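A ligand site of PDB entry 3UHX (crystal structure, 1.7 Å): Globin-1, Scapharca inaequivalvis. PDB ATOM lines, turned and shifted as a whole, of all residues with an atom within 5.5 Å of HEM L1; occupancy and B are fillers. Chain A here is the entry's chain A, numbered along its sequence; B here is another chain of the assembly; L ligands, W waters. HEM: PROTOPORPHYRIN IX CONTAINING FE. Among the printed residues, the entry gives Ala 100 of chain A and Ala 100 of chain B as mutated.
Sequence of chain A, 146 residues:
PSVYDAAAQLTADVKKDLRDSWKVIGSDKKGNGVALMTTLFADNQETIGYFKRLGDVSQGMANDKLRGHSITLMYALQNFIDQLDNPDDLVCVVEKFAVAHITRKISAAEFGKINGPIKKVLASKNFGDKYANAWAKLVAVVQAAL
An iron atom (FE) of HEM L1 is bound by a ring nitrogen (NE2) of His 101. NH2 of Arg 104 lies within salt-bridge range of O1A of HEM L1 (2.6 Å). NH2 of Arg 53 lies within salt-bridge range of O2D of HEM L1, 2.7 Å away. O2D of HEM L1 lies within salt-bridge range of NZ of Lys 96 of chain B (2.7 Å).
ND1 of His 101 lies within hydrogen-bond range of O of Phe 97 (3.2 Å). N of Ile 106 is in hydrogen-bond range of O of His 101. NH1 of Arg 104 is in hydrogen-bond range of O of Ala 100 of chain A (3.1 Å). The side-chain amino group (NZ) of Lys 96 of chain B sits at hydrogen-bond distance from a ring nitrogen (ND1) of His 69 (2.9 Å). The side-chain hydroxyl of Tyr 50 lies within hydrogen-bond range of the side-chain carboxylate of Glu 110 (2.7 Å).
Merely in contact with HEM L1: Tyr 50, Ala 100 of chain A, Phe 51, Phe 97, Phe 111, Leu 73, His 69, Leu 54, Ile 114, Glu 110, Ala 76, Leu 77, Thr 72 and Ile 106. Hydrophobic or aromatic side chains within 4 Å of HEM L1: Phe 51, Leu 54, His 69, Leu 73, Ala 76, Leu 77, Phe 97, Ala 100 of chain A, His 101, Ile 106, Phe 111 and Ile 114. Within 4 Å of HEM L1: Tyr 50, Phe 51, Arg 53, Leu 54, His 69, Thr 72, Leu 73, Ala 76, Leu 77, Phe 97, Ala 100 of chain A, His 101, Arg 104, Ile 106, Glu 110, Phe 111, Ile 114 and Lys 96 of chain B. The nearest printed residue that does not touch HEM L1 is Thr 47 (4.2 Å).
Water W1 lies within hydrogen-bond range of O2A of HEM L1 (2.7 Å) and O of Phe 97 (3.1 Å). Water W6 lies within hydrogen-bond range of O1A of HEM L1 (2.7 Å), NZ of Lys 96 of chain B (3.1 Å) and NH2 of Arg 104 (3.3 Å). Water W4 lies within hydrogen-bond range of O1A of HEM L1 (2.8 Å) and O1A of HEM L2 (2.9 Å). Water W3 lies within hydrogen-bond range of O of Tyr 50 (2.9 Å), O1D of HEM L1 (3.1 Å) and N of Arg 53 (3.5 Å).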
ATOM      1  N   LEU A  36      11.470  10.823  26.607  1.00  0.00           N
ATOM      2  CA  LEU A  36      11.146  12.127  26.060  1.00  0.00           C
ATOM      3  C   LEU A  36      12.025  12.432  24.843  1.00  0.00           C
ATOM      4  O   LEU A  36      11.533  12.862  23.795  1.00  0.00           O
ATOM      5  CB  LEU A  36      11.338  13.187  27.135  1.00  0.00           C
ATOM      6  CG  LEU A  36      10.595  14.510  27.001  1.00  0.00           C
ATOM      7  CD1 LEU A  36       9.099  14.247  26.865  1.00  0.00           C
ATOM      8  CD2 LEU A  36      10.872  15.381  28.225  1.00  0.00           C
ATOM      9  N   LEU A  40      11.120  12.568  20.725  1.00  0.00           N
ATOM     10  CA  LEU A  40      11.376  13.771  19.951  1.00  0.00           C
ATOM     11  C   LEU A  40      12.098  13.419  18.656  1.00  0.00           C
ATOM     12  O   LEU A  40      11.723  13.871  17.577  1.00  0.00           O
ATOM     13  CB  LEU A  40      12.234  14.755  20.739  1.00  0.00           C
ATOM     14  CG  LEU A  40      12.733  15.985  19.968  1.00  0.00           C
ATOM     15  CD1 LEU A  40      11.551  16.831  19.541  1.00  0.00           C
ATOM     16  CD2 LEU A  40      13.691  16.783  20.831  1.00  0.00           C
ATOM     17  N   THR A  47      15.460  17.313  14.027  1.00  0.00           N
ATOM     18  CA  THR A  47      16.062  17.937  15.196  1.00  0.00           C
ATOM     19  C   THR A  47      17.341  17.232  15.618  1.00  0.00           C
ATOM     20  O   THR A  47      18.120  17.752  16.416  1.00  0.00           O
ATOM     21  CB  THR A  47      15.089  17.956  16.408  1.00  0.00           C
ATOM     22  OG1 THR A  47      14.767  16.605  16.781  1.00  0.00           O
ATOM     23  CG2 THR A  47      13.817  18.713  16.066  1.00  0.00           C
ATOM     24  N   TYR A  50      20.927  18.923  15.671  1.00  0.00           N
ATOM     25  CA  TYR A  50      21.374  19.748  16.791  1.00  0.00           C
ATOM     26  C   TYR A  50      22.114  18.940  17.847  1.00  0.00           C
ATOM     27  O   TYR A  50      22.861  19.494  18.662  1.00  0.00           O
ATOM     28  CB  TYR A  50      20.169  20.415  17.459  1.00  0.00           C
ATOM     29  CG  TYR A  50      19.471  21.471  16.627  1.00  0.00           C
ATOM     30  CD1 TYR A  50      20.110  22.675  16.332  1.00  0.00           C
ATOM     31  CD2 TYR A  50      18.168  21.286  16.167  1.00  0.00           C
ATOM     32  CE1 TYR A  50      19.468  23.674  15.600  1.00  0.00           C
ATOM     33  CE2 TYR A  50      17.521  22.273  15.439  1.00  0.00           C
ATOM     34  CZ  TYR A  50      18.169  23.463  15.167  1.00  0.00           C
ATOM     35  OH  TYR A  50      17.523  24.452  14.448  1.00  0.00           O
ATOM     36  N   PHE A  51      21.919  17.624  17.821  1.00  0.00           N
ATOM     37  CA  PHE A  51      22.531  16.737  18.810  1.00  0.00           C
ATOM     38  C   PHE A  51      23.668  15.865  18.263  1.00  0.00           C
ATOM     39  O   PHE A  51      23.845  14.729  18.695  1.00  0.00           O
ATOM     40  CB  PHE A  51      21.448  15.843  19.419  1.00  0.00           C
ATOM     41  CG  PHE A  51      20.365  16.614  20.128  1.00  0.00           C
ATOM     42  CD1 PHE A  51      20.518  16.966  21.465  1.00  0.00           C
ATOM     43  CD2 PHE A  51      19.205  16.983  19.463  1.00  0.00           C
ATOM     44  CE1 PHE A  51      19.514  17.675  22.128  1.00  0.00           C
ATOM     45  CE2 PHE A  51      18.200  17.689  20.116  1.00  0.00           C
ATOM     46  CZ  PHE A  51      18.353  18.041  21.452  1.00  0.00           C
ATOM     47  N   ARG A  53      26.795  15.875  18.777  1.00  0.00           N
ATOM     48  CA  ARG A  53      27.733  15.449  19.818  1.00  0.00           C
ATOM     49  C   ARG A  53      27.320  14.168  20.538  1.00  0.00           C
ATOM     50  O   ARG A  53      28.178  13.423  21.014  1.00  0.00           O
ATOM     51  CB  ARG A  53      27.911  16.569  20.838  1.00  0.00           C
ATOM     52  CG  ARG A  53      29.050  16.330  21.828  1.00  0.00           C
ATOM     53  CD  ARG A  53      29.030  17.361  22.938  1.00  0.00           C
ATOM     54  NE  ARG A  53      27.955  17.098  23.889  1.00  0.00           N
ATOM     55  CZ  ARG A  53      27.989  16.138  24.815  1.00  0.00           C
ATOM     56  NH1 ARG A  53      29.051  15.354  24.911  1.00  0.00           N
ATOM     57  NH2 ARG A  53      26.961  15.959  25.636  1.00  0.00           N
ATOM     58  N   LEU A  54      26.020  13.921  20.623  1.00  0.00           N
ATOM     59  CA  LEU A  54      25.521  12.730  21.312  1.00  0.00           C
ATOM     60  C   LEU A  54      25.797  11.409  20.593  1.00  0.00           C
ATOM     61  O   LEU A  54      25.744  10.353  21.211  1.00  0.00           O
ATOM     62  CB  LEU A  54      24.012  12.867  21.568  1.00  0.00           C
ATOM     63  CG  LEU A  54      23.576  13.761  22.734  1.00  0.00           C
ATOM     64  CD1 LEU A  54      24.287  15.106  22.665  1.00  0.00           C
ATOM     65  CD2 LEU A  54      22.070  13.943  22.688  1.00  0.00           C
ATOM     66  N   HIS A  69      22.460  13.466  28.991  1.00  0.00           N
ATOM     67  CA  HIS A  69      21.693  14.639  28.586  1.00  0.00           C
ATOM     68  C   HIS A  69      20.249  14.536  29.059  1.00  0.00           C
ATOM     69  O   HIS A  69      19.692  15.511  29.587  1.00  0.00           O
ATOM     70  CB  HIS A  69      21.692  14.770  27.060  1.00  0.00           C
ATOM     71  CG  HIS A  69      20.764  15.823  26.559  1.00  0.00           C
ATOM     72  ND1 HIS A  69      21.053  17.159  26.651  1.00  0.00           N
ATOM     73  CD2 HIS A  69      19.518  15.670  26.022  1.00  0.00           C
ATOM     74  CE1 HIS A  69      20.002  17.789  26.187  1.00  0.00           C
ATOM     75  NE2 HIS A  69      19.038  16.932  25.786  1.00  0.00           N
ATOM     76  N   THR A  72      19.829  15.068  32.781  1.00  0.00           N
ATOM     77  CA  THR A  72      20.063  16.480  33.048  1.00  0.00           C
ATOM     78  C   THR A  72      18.887  17.357  32.654  1.00  0.00           C
ATOM     79  O   THR A  72      18.542  18.313  33.357  1.00  0.00           O
ATOM     80  CB  THR A  72      21.334  16.955  32.310  1.00  0.00           C
ATOM     81  OG1 THR A  72      22.460  16.224  32.830  1.00  0.00           O
ATOM     82  CG2 THR A  72      21.560  18.441  32.518  1.00  0.00           C
ATOM     83  N   LEU A  73      18.267  17.031  31.528  1.00  0.00           N
ATOM     84  CA  LEU A  73      17.115  17.789  31.036  1.00  0.00           C
ATOM     85  C   LEU A  73      15.984  17.772  32.069  1.00  0.00           C
ATOM     86  O   LEU A  73      15.293  18.780  32.255  1.00  0.00           O
ATOM     87  CB  LEU A  73      16.624  17.184  29.712  1.00  0.00           C
ATOM     88  CG  LEU A  73      15.276  17.629  29.124  1.00  0.00           C
ATOM     89  CD1 LEU A  73      15.303  17.424  27.625  1.00  0.00           C
ATOM     90  CD2 LEU A  73      14.135  16.848  29.765  1.00  0.00           C
ATOM     91  N   ALA A  76      16.061  20.420  34.794  1.00  0.00           N
ATOM     92  CA  ALA A  76      15.724  21.778  34.380  1.00  0.00           C
ATOM     93  C   ALA A  76      14.215  21.899  34.609  1.00  0.00           C
ATOM     94  O   ALA A  76      13.725  22.949  35.028  1.00  0.00           O
ATOM     95  CB  ALA A  76      16.055  21.983  32.896  1.00  0.00           C
ATOM     96  N   LEU A  77      13.485  20.822  34.325  1.00  0.00           N
ATOM     97  CA  LEU A  77      12.039  20.821  34.524  1.00  0.00           C
ATOM     98  C   LEU A  77      11.766  20.843  36.027  1.00  0.00           C
ATOM     99  O   LEU A  77      10.819  21.482  36.482  1.00  0.00           O
ATOM    100  CB  LEU A  77      11.409  19.587  33.880  1.00  0.00           C
ATOM    101  CG  LEU A  77      11.450  19.527  32.354  1.00  0.00           C
ATOM    102  CD1 LEU A  77      10.745  18.269  31.872  1.00  0.00           C
ATOM    103  CD2 LEU A  77      10.782  20.765  31.774  1.00  0.00           C
ATOM    104  N   PHE A  80      12.095  24.409  37.124  1.00  0.00           N
ATOM    105  CA  PHE A  80      10.916  25.205  36.771  1.00  0.00           C
ATOM    106  C   PHE A  80       9.746  24.956  37.721  1.00  0.00           C
ATOM    107  O   PHE A  80       9.118  25.893  38.207  1.00  0.00           O
ATOM    108  CB  PHE A  80      10.456  24.914  35.346  1.00  0.00           C
ATOM    109  CG  PHE A  80      11.474  25.231  34.285  1.00  0.00           C
ATOM    110  CD1 PHE A  80      12.497  26.148  34.519  1.00  0.00           C
ATOM    111  CD2 PHE A  80      11.403  24.631  33.030  1.00  0.00           C
ATOM    112  CE1 PHE A  80      13.424  26.461  33.532  1.00  0.00           C
ATOM    113  CE2 PHE A  80      12.324  24.930  32.037  1.00  0.00           C
ATOM    114  CZ  PHE A  80      13.338  25.846  32.283  1.00  0.00           C
ATOM    115  N   PHE A  97      18.047  29.701  31.566  1.00  0.00           N
ATOM    116  CA  PHE A  97      17.940  28.497  30.765  1.00  0.00           C
ATOM    117  C   PHE A  97      17.975  28.804  29.263  1.00  0.00           C
ATOM    118  O   PHE A  97      18.592  28.075  28.500  1.00  0.00           O
ATOM    119  CB  PHE A  97      16.632  27.793  31.139  1.00  0.00           C
ATOM    120  CG  PHE A  97      16.257  26.672  30.217  1.00  0.00           C
ATOM    121  CD1 PHE A  97      15.585  26.921  29.029  1.00  0.00           C
ATOM    122  CD2 PHE A  97      16.568  25.367  30.558  1.00  0.00           C
ATOM    123  CE1 PHE A  97      15.230  25.877  28.179  1.00  0.00           C
ATOM    124  CE2 PHE A  97      16.227  24.320  29.717  1.00  0.00           C
ATOM    125  CZ  PHE A  97      15.555  24.569  28.530  1.00  0.00           C
ATOM    126  N   ALA A 100      21.810  29.478  26.814  1.00  0.00           N
ATOM    127  CA  ALA A 100      22.476  28.430  26.060  1.00  0.00           C
ATOM    128  C   ALA A 100      21.698  27.993  24.826  1.00  0.00           C
ATOM    129  O   ALA A 100      22.296  27.692  23.795  1.00  0.00           O
ATOM    130  CB  ALA A 100      22.744  27.223  26.964  1.00  0.00           C
ATOM    131  N   HIS A 101      20.378  27.970  24.910  1.00  0.00           N
ATOM    132  CA  HIS A 101      19.587  27.552  23.746  1.00  0.00           C
ATOM    133  C   HIS A 101      19.565  28.658  22.689  1.00  0.00           C
ATOM    134  O   HIS A 101      19.433  28.366  21.501  1.00  0.00           O
ATOM    135  CB  HIS A 101      18.173  27.176  24.167  1.00  0.00           C
ATOM    136  CG  HIS A 101      18.094  25.883  24.940  1.00  0.00           C
ATOM    137  ND1 HIS A 101      18.448  25.766  26.262  1.00  0.00           N
ATOM    138  CD2 HIS A 101      17.767  24.626  24.533  1.00  0.00           C
ATOM    139  CE1 HIS A 101      18.332  24.467  26.616  1.00  0.00           C
ATOM    140  NE2 HIS A 101      17.922  23.743  25.591  1.00  0.00           N
ATOM    141  N   ARG A 104      22.539  28.454  20.598  1.00  0.00           N
ATOM    142  CA  ARG A 104      22.550  27.259  19.748  1.00  0.00           C
ATOM    143  C   ARG A 104      21.615  27.519  18.581  1.00  0.00           C
ATOM    144  O   ARG A 104      21.415  26.664  17.727  1.00  0.00           O
ATOM    145  CB  ARG A 104      22.045  26.033  20.498  1.00  0.00           C
ATOM    146  CG  ARG A 104      22.982  25.494  21.535  1.00  0.00           C
ATOM    147  CD  ARG A 104      22.466  24.150  22.035  1.00  0.00           C
ATOM    148  NE  ARG A 104      23.353  23.585  23.044  1.00  0.00           N
ATOM    149  CZ  ARG A 104      23.306  23.884  24.326  1.00  0.00           C
ATOM    150  NH1 ARG A 104      22.406  24.742  24.783  1.00  0.00           N
ATOM    151  NH2 ARG A 104      24.180  23.337  25.166  1.00  0.00           N
ATOM    152  N   ILE A 106      18.284  27.969  18.687  1.00  0.00           N
ATOM    153  CA  ILE A 106      17.060  27.192  18.777  1.00  0.00           C
ATOM    154  C   ILE A 106      15.925  28.186  18.909  1.00  0.00           C
ATOM    155  O   ILE A 106      15.820  28.894  19.912  1.00  0.00           O
ATOM    156  CB  ILE A 106      17.054  26.262  20.012  1.00  0.00           C
ATOM    157  CG1 ILE A 106      18.242  25.297  19.969  1.00  0.00           C
ATOM    158  CG2 ILE A 106      15.738  25.505  20.068  1.00  0.00           C
ATOM    159  CD1 ILE A 106      18.274  24.394  18.744  1.00  0.00           C
ATOM    160  N   GLU A 110      11.135  25.865  17.102  1.00  0.00           N
ATOM    161  CA  GLU A 110      11.878  24.616  17.218  1.00  0.00           C
ATOM    162  C   GLU A 110      11.850  24.041  18.629  1.00  0.00           C
ATOM    163  O   GLU A 110      11.991  22.834  18.823  1.00  0.00           O
ATOM    164  CB  GLU A 110      13.338  24.810  16.783  1.00  0.00           C
ATOM    165  CG  GLU A 110      13.510  25.058  15.299  1.00  0.00           C
ATOM    166  CD  GLU A 110      14.000  23.828  14.572  1.00  0.00           C
ATOM    167  OE1 GLU A 110      13.419  22.728  14.761  1.00  0.00           O
ATOM    168  OE2 GLU A 110      14.975  23.949  13.803  1.00  0.00           O
ATOM    169  N   PHE A 111      11.667  24.910  19.612  1.00  0.00           N
ATOM    170  CA  PHE A 111      11.617  24.466  21.004  1.00  0.00           C
ATOM    171  C   PHE A 111      10.255  23.840  21.273  1.00  0.00           C
ATOM    172  O   PHE A 111      10.148  22.849  22.007  1.00  0.00           O
ATOM    173  CB  PHE A 111      11.824  25.641  21.955  1.00  0.00           C
ATOM    174  CG  PHE A 111      12.099  25.220  23.372  1.00  0.00           C
ATOM    175  CD1 PHE A 111      13.383  24.891  23.783  1.00  0.00           C
ATOM    176  CD2 PHE A 111      11.068  25.139  24.304  1.00  0.00           C
ATOM    177  CE1 PHE A 111      13.639  24.486  25.095  1.00  0.00           C
ATOM    178  CE2 PHE A 111      11.315  24.731  25.617  1.00  0.00           C
ATOM    179  CZ  PHE A 111      12.606  24.400  26.008  1.00  0.00           C
ATOM    180  N   ILE A 114       8.875  20.036  21.377  1.00  0.00           N
ATOM    181  CA  ILE A 114       8.962  19.166  22.544  1.00  0.00           C
ATOM    182  C   ILE A 114       7.574  18.897  23.123  1.00  0.00           C
ATOM    183  O   ILE A 114       7.389  17.971  23.913  1.00  0.00           O
ATOM    184  CB  ILE A 114       9.858  19.783  23.646  1.00  0.00           C
ATOM    185  CG1 ILE A 114      10.272  18.700  24.636  1.00  0.00           C
ATOM    186  CG2 ILE A 114       9.109  20.890  24.375  1.00  0.00           C
ATOM    187  CD1 ILE A 114      11.156  17.631  24.036  1.00  0.00           C
ATOM    188  N   ILE A 118       6.119  15.429  25.127  1.00  0.00           N
ATOM    189  CA  ILE A 118       5.613  15.599  26.480  1.00  0.00           C
ATOM    190  C   ILE A 118       4.194  15.049  26.581  1.00  0.00           C
ATOM    191  O   ILE A 118       3.853  14.363  27.530  1.00  0.00           O
ATOM    192  CB  ILE A 118       5.651  17.080  26.921  1.00  0.00           C
ATOM    193  CG1 ILE A 118       7.105  17.535  27.056  1.00  0.00           C
ATOM    194  CG2 ILE A 118       4.916  17.257  28.250  1.00  0.00           C
ATOM    195  CD1 ILE A 118       7.277  18.969  27.523  1.00  0.00           C
ATOM    196  N   VAL A 139       5.916  25.494  28.717  1.00  0.00           N
ATOM    197  CA  VAL A 139       6.838  25.548  27.598  1.00  0.00           C
ATOM    198  C   VAL A 139       6.715  26.901  26.909  1.00  0.00           C
ATOM    199  O   VAL A 139       7.704  27.456  26.416  1.00  0.00           O
ATOM    200  CB  VAL A 139       6.546  24.411  26.576  1.00  0.00           C
ATOM    201  CG1 VAL A 139       7.351  24.617  25.300  1.00  0.00           C
ATOM    202  CG2 VAL A 139       6.902  23.069  27.201  1.00  0.00           C
ATOM    203  N   LYS B  96      28.508  15.192  30.978  1.00  0.00           N
ATOM    204  CA  LYS B  96      27.561  16.068  30.284  1.00  0.00           C
ATOM    205  C   LYS B  96      27.736  17.484  30.828  1.00  0.00           C
ATOM    206  O   LYS B  96      27.799  18.465  30.081  1.00  0.00           O
ATOM    207  CB  LYS B  96      26.123  15.592  30.526  1.00  0.00           C
ATOM    208  CG  LYS B  96      25.030  16.651  30.326  1.00  0.00           C
ATOM    209  CD  LYS B  96      24.876  17.107  28.875  1.00  0.00           C
ATOM    210  CE  LYS B  96      23.771  18.154  28.751  1.00  0.00           C
ATOM    211  NZ  LYS B  96      23.491  18.563  27.339  1.00  0.00           N
ATOM    212  N   VAL B  99      30.966  19.415  29.571  1.00  0.00           N
ATOM    213  CA  VAL B  99      30.968  19.908  28.194  1.00  0.00           C
ATOM    214  C   VAL B  99      30.940  21.432  28.074  1.00  0.00           C
ATOM    215  O   VAL B  99      31.819  22.028  27.461  1.00  0.00           O
ATOM    216  CB  VAL B  99      29.791  19.317  27.403  1.00  0.00           C
ATOM    217  CG1 VAL B  99      29.668  20.003  26.047  1.00  0.00           C
ATOM    218  CG2 VAL B  99      30.001  17.824  27.212  1.00  0.00           C
ATOM    219  N   ALA B 100      29.921  22.054  28.666  1.00  0.00           N
ATOM    220  CA  ALA B 100      29.779  23.506  28.599  1.00  0.00           C
ATOM    221  C   ALA B 100      30.905  24.237  29.311  1.00  0.00           C
ATOM    222  O   ALA B 100      31.309  25.315  28.880  1.00  0.00           O
ATOM    223  CB  ALA B 100      28.419  23.923  29.172  1.00  0.00           C
HETATM  224  CHA HEM L   1      21.183  21.147  26.280  1.00  0.00           C
HETATM  225  CHB HEM L   1      17.087  21.104  28.806  1.00  0.00           C
HETATM  226  CHC HEM L   1      14.532  21.150  24.706  1.00  0.00           C
HETATM  227  CHD HEM L   1      18.629  21.395  22.193  1.00  0.00           C
HETATM  228  C1A HEM L   1      20.286  21.301  27.334  1.00  0.00           C
HETATM  229  C2A HEM L   1      20.664  21.290  28.751  1.00  0.00           C
HETATM  230  C3A HEM L   1      19.499  21.249  29.442  1.00  0.00           C
HETATM  231  C4A HEM L   1      18.423  21.253  28.471  1.00  0.00           C
HETATM  232  CMA HEM L   1      19.357  21.308  30.961  1.00  0.00           C
HETATM  233  CAA HEM L   1      22.057  21.367  29.371  1.00  0.00           C
HETATM  234  CBA HEM L   1      22.457  22.807  29.640  1.00  0.00           C
HETATM  235  CGA HEM L   1      22.659  23.603  28.361  1.00  0.00           C
HETATM  236  O1A HEM L   1      23.718  23.442  27.722  1.00  0.00           O
HETATM  237  O2A HEM L   1      21.740  24.362  27.983  1.00  0.00           O
HETATM  238  C1B HEM L   1      16.033  21.119  27.901  1.00  0.00           C
HETATM  239  C2B HEM L   1      14.631  21.030  28.292  1.00  0.00           C
HETATM  240  C3B HEM L   1      13.906  21.041  27.139  1.00  0.00           C
HETATM  241  C4B HEM L   1      14.877  21.155  26.050  1.00  0.00           C
HETATM  242  CMB HEM L   1      14.100  21.026  29.722  1.00  0.00           C
HETATM  243  CAB HEM L   1      12.514  21.043  26.998  1.00  0.00           C
HETATM  244  CBB HEM L   1      11.571  20.270  27.756  1.00  0.00           C
HETATM  245  C1C HEM L   1      15.439  21.291  23.671  1.00  0.00           C
HETATM  246  C2C HEM L   1      15.066  21.241  22.269  1.00  0.00           C
HETATM  247  C3C HEM L   1      16.216  21.303  21.544  1.00  0.00           C
HETATM  248  C4C HEM L   1      17.292  21.443  22.521  1.00  0.00           C
HETATM  249  CMC HEM L   1      13.631  21.166  21.758  1.00  0.00           C
HETATM  250  CAC HEM L   1      16.407  21.244  20.153  1.00  0.00           C
HETATM  251  CBC HEM L   1      15.428  21.120  19.097  1.00  0.00           C
HETATM  252  C1D HEM L   1      19.669  21.274  23.094  1.00  0.00           C
HETATM  253  C2D HEM L   1      21.024  20.924  22.712  1.00  0.00           C
HETATM  254  C3D HEM L   1      21.723  20.799  23.845  1.00  0.00           C
HETATM  255  C4D HEM L   1      20.811  21.098  24.939  1.00  0.00           C
HETATM  256  CMD HEM L   1      21.596  20.676  21.319  1.00  0.00           C
HETATM  257  CAD HEM L   1      23.180  20.371  23.927  1.00  0.00           C
HETATM  258  CBD HEM L   1      23.309  18.857  23.928  1.00  0.00           C
HETATM  259  CGD HEM L   1      24.735  18.385  24.138  1.00  0.00           C
HETATM  260  O1D HEM L   1      25.569  18.598  23.241  1.00  0.00           O
HETATM  261  O2D HEM L   1      25.013  17.812  25.207  1.00  0.00           O
HETATM  262  NA  HEM L   1      18.915  21.356  27.188  1.00  0.00           N
HETATM  263  NB  HEM L   1      16.174  21.252  26.522  1.00  0.00           N
HETATM  264  NC  HEM L   1      16.806  21.447  23.829  1.00  0.00           N
HETATM  265  ND  HEM L   1      19.526  21.338  24.466  1.00  0.00           N
HETATM  266 FE   HEM L   1      17.859  21.689  25.511  1.00  0.00          FE
HETATM  267  CHA HEM L   2      27.061  27.932  33.960  1.00  0.00           C
HETATM  268  CHB HEM L   2      26.906  24.786  37.615  1.00  0.00           C
HETATM  269  CHC HEM L   2      31.287  26.217  39.040  1.00  0.00           C
HETATM  270  CHD HEM L   2      31.523  29.235  35.281  1.00  0.00           C
HETATM  271  C1A HEM L   2      26.704  26.854  34.748  1.00  0.00           C
HETATM  272  C2A HEM L   2      25.440  26.138  34.663  1.00  0.00           C
HETATM  273  C3A HEM L   2      25.426  25.239  35.673  1.00  0.00           C
HETATM  274  C4A HEM L   2      26.629  25.423  36.416  1.00  0.00           C
HETATM  275  CMA HEM L   2      24.329  24.190  35.907  1.00  0.00           C
HETATM  276  CAA HEM L   2      24.380  26.260  33.577  1.00  0.00           C
HETATM  277  CBA HEM L   2      24.617  25.254  32.454  1.00  0.00           C
HETATM  278  CGA HEM L   2      25.871  25.568  31.654  1.00  0.00           C
HETATM  279  O1A HEM L   2      25.835  26.516  30.845  1.00  0.00           O
HETATM  280  O2A HEM L   2      26.894  24.887  31.853  1.00  0.00           O
HETATM  281  C1B HEM L   2      28.102  24.901  38.303  1.00  0.00           C
HETATM  282  C2B HEM L   2      28.373  24.155  39.530  1.00  0.00           C
HETATM  283  C3B HEM L   2      29.607  24.560  39.965  1.00  0.00           C
HETATM  284  C4B HEM L   2      30.092  25.518  38.952  1.00  0.00           C
HETATM  285  CMB HEM L   2      27.482  23.078  40.138  1.00  0.00           C
HETATM  286  CAB HEM L   2      30.322  24.129  41.078  1.00  0.00           C
HETATM  287  CBB HEM L   2      29.823  23.522  42.288  1.00  0.00           C
HETATM  288  C1C HEM L   2      31.767  27.106  38.085  1.00  0.00           C
HETATM  289  C2C HEM L   2      33.012  27.846  38.219  1.00  0.00           C
HETATM  290  C3C HEM L   2      33.116  28.671  37.142  1.00  0.00           C
HETATM  291  C4C HEM L   2      31.908  28.442  36.349  1.00  0.00           C
HETATM  292  CMC HEM L   2      33.985  27.714  39.391  1.00  0.00           C
HETATM  293  CAC HEM L   2      34.175  29.513  36.777  1.00  0.00           C
HETATM  294  CBC HEM L   2      35.107  30.191  37.652  1.00  0.00           C
HETATM  295  C1D HEM L   2      30.307  29.162  34.627  1.00  0.00           C
HETATM  296  C2D HEM L   2      29.872  30.139  33.656  1.00  0.00           C
HETATM  297  C3D HEM L   2      28.606  29.816  33.318  1.00  0.00           C
HETATM  298  C4D HEM L   2      28.281  28.598  34.053  1.00  0.00           C
HETATM  299  CMD HEM L   2      30.659  31.328  33.117  1.00  0.00           C
HETATM  300  CAD HEM L   2      27.695  30.661  32.441  1.00  0.00           C
HETATM  301  CBD HEM L   2      26.999  31.743  33.263  1.00  0.00           C
HETATM  302  CGD HEM L   2      26.047  32.593  32.452  1.00  0.00           C
HETATM  303  O1D HEM L   2      26.508  33.411  31.631  1.00  0.00           O
HETATM  304  O2D HEM L   2      24.813  32.424  32.623  1.00  0.00           O
HETATM  305  NA  HEM L   2      27.478  26.348  35.799  1.00  0.00           N
HETATM  306  NB  HEM L   2      29.178  25.677  37.900  1.00  0.00           N
HETATM  307  NC  HEM L   2      31.113  27.452  36.902  1.00  0.00           N
HETATM  308  ND  HEM L   2      29.319  28.221  34.893  1.00  0.00           N
HETATM  309 FE   HEM L   2      29.408  26.677  36.173  1.00  0.00          FE
HETATM  310  O   HOH W   1      20.453  25.895  29.736  1.00  0.00           O
HETATM  311  O   HOH W   2      23.497  22.241  18.934  1.00  0.00           O
HETATM  312  O   HOH W   3      25.165  18.619  20.175  1.00  0.00           O
HETATM  313  O   HOH W   4      25.507  25.492  28.160  1.00  0.00           O
HETATM  314  O   HOH W   5      25.191  20.717  30.232  1.00  0.00           O
HETATM  315  O   HOH W   6      25.147  21.169  27.460  1.00  0.00           O
HETATM  316  O   HOH W   7      16.740  18.436  24.658  1.00  0.00           O
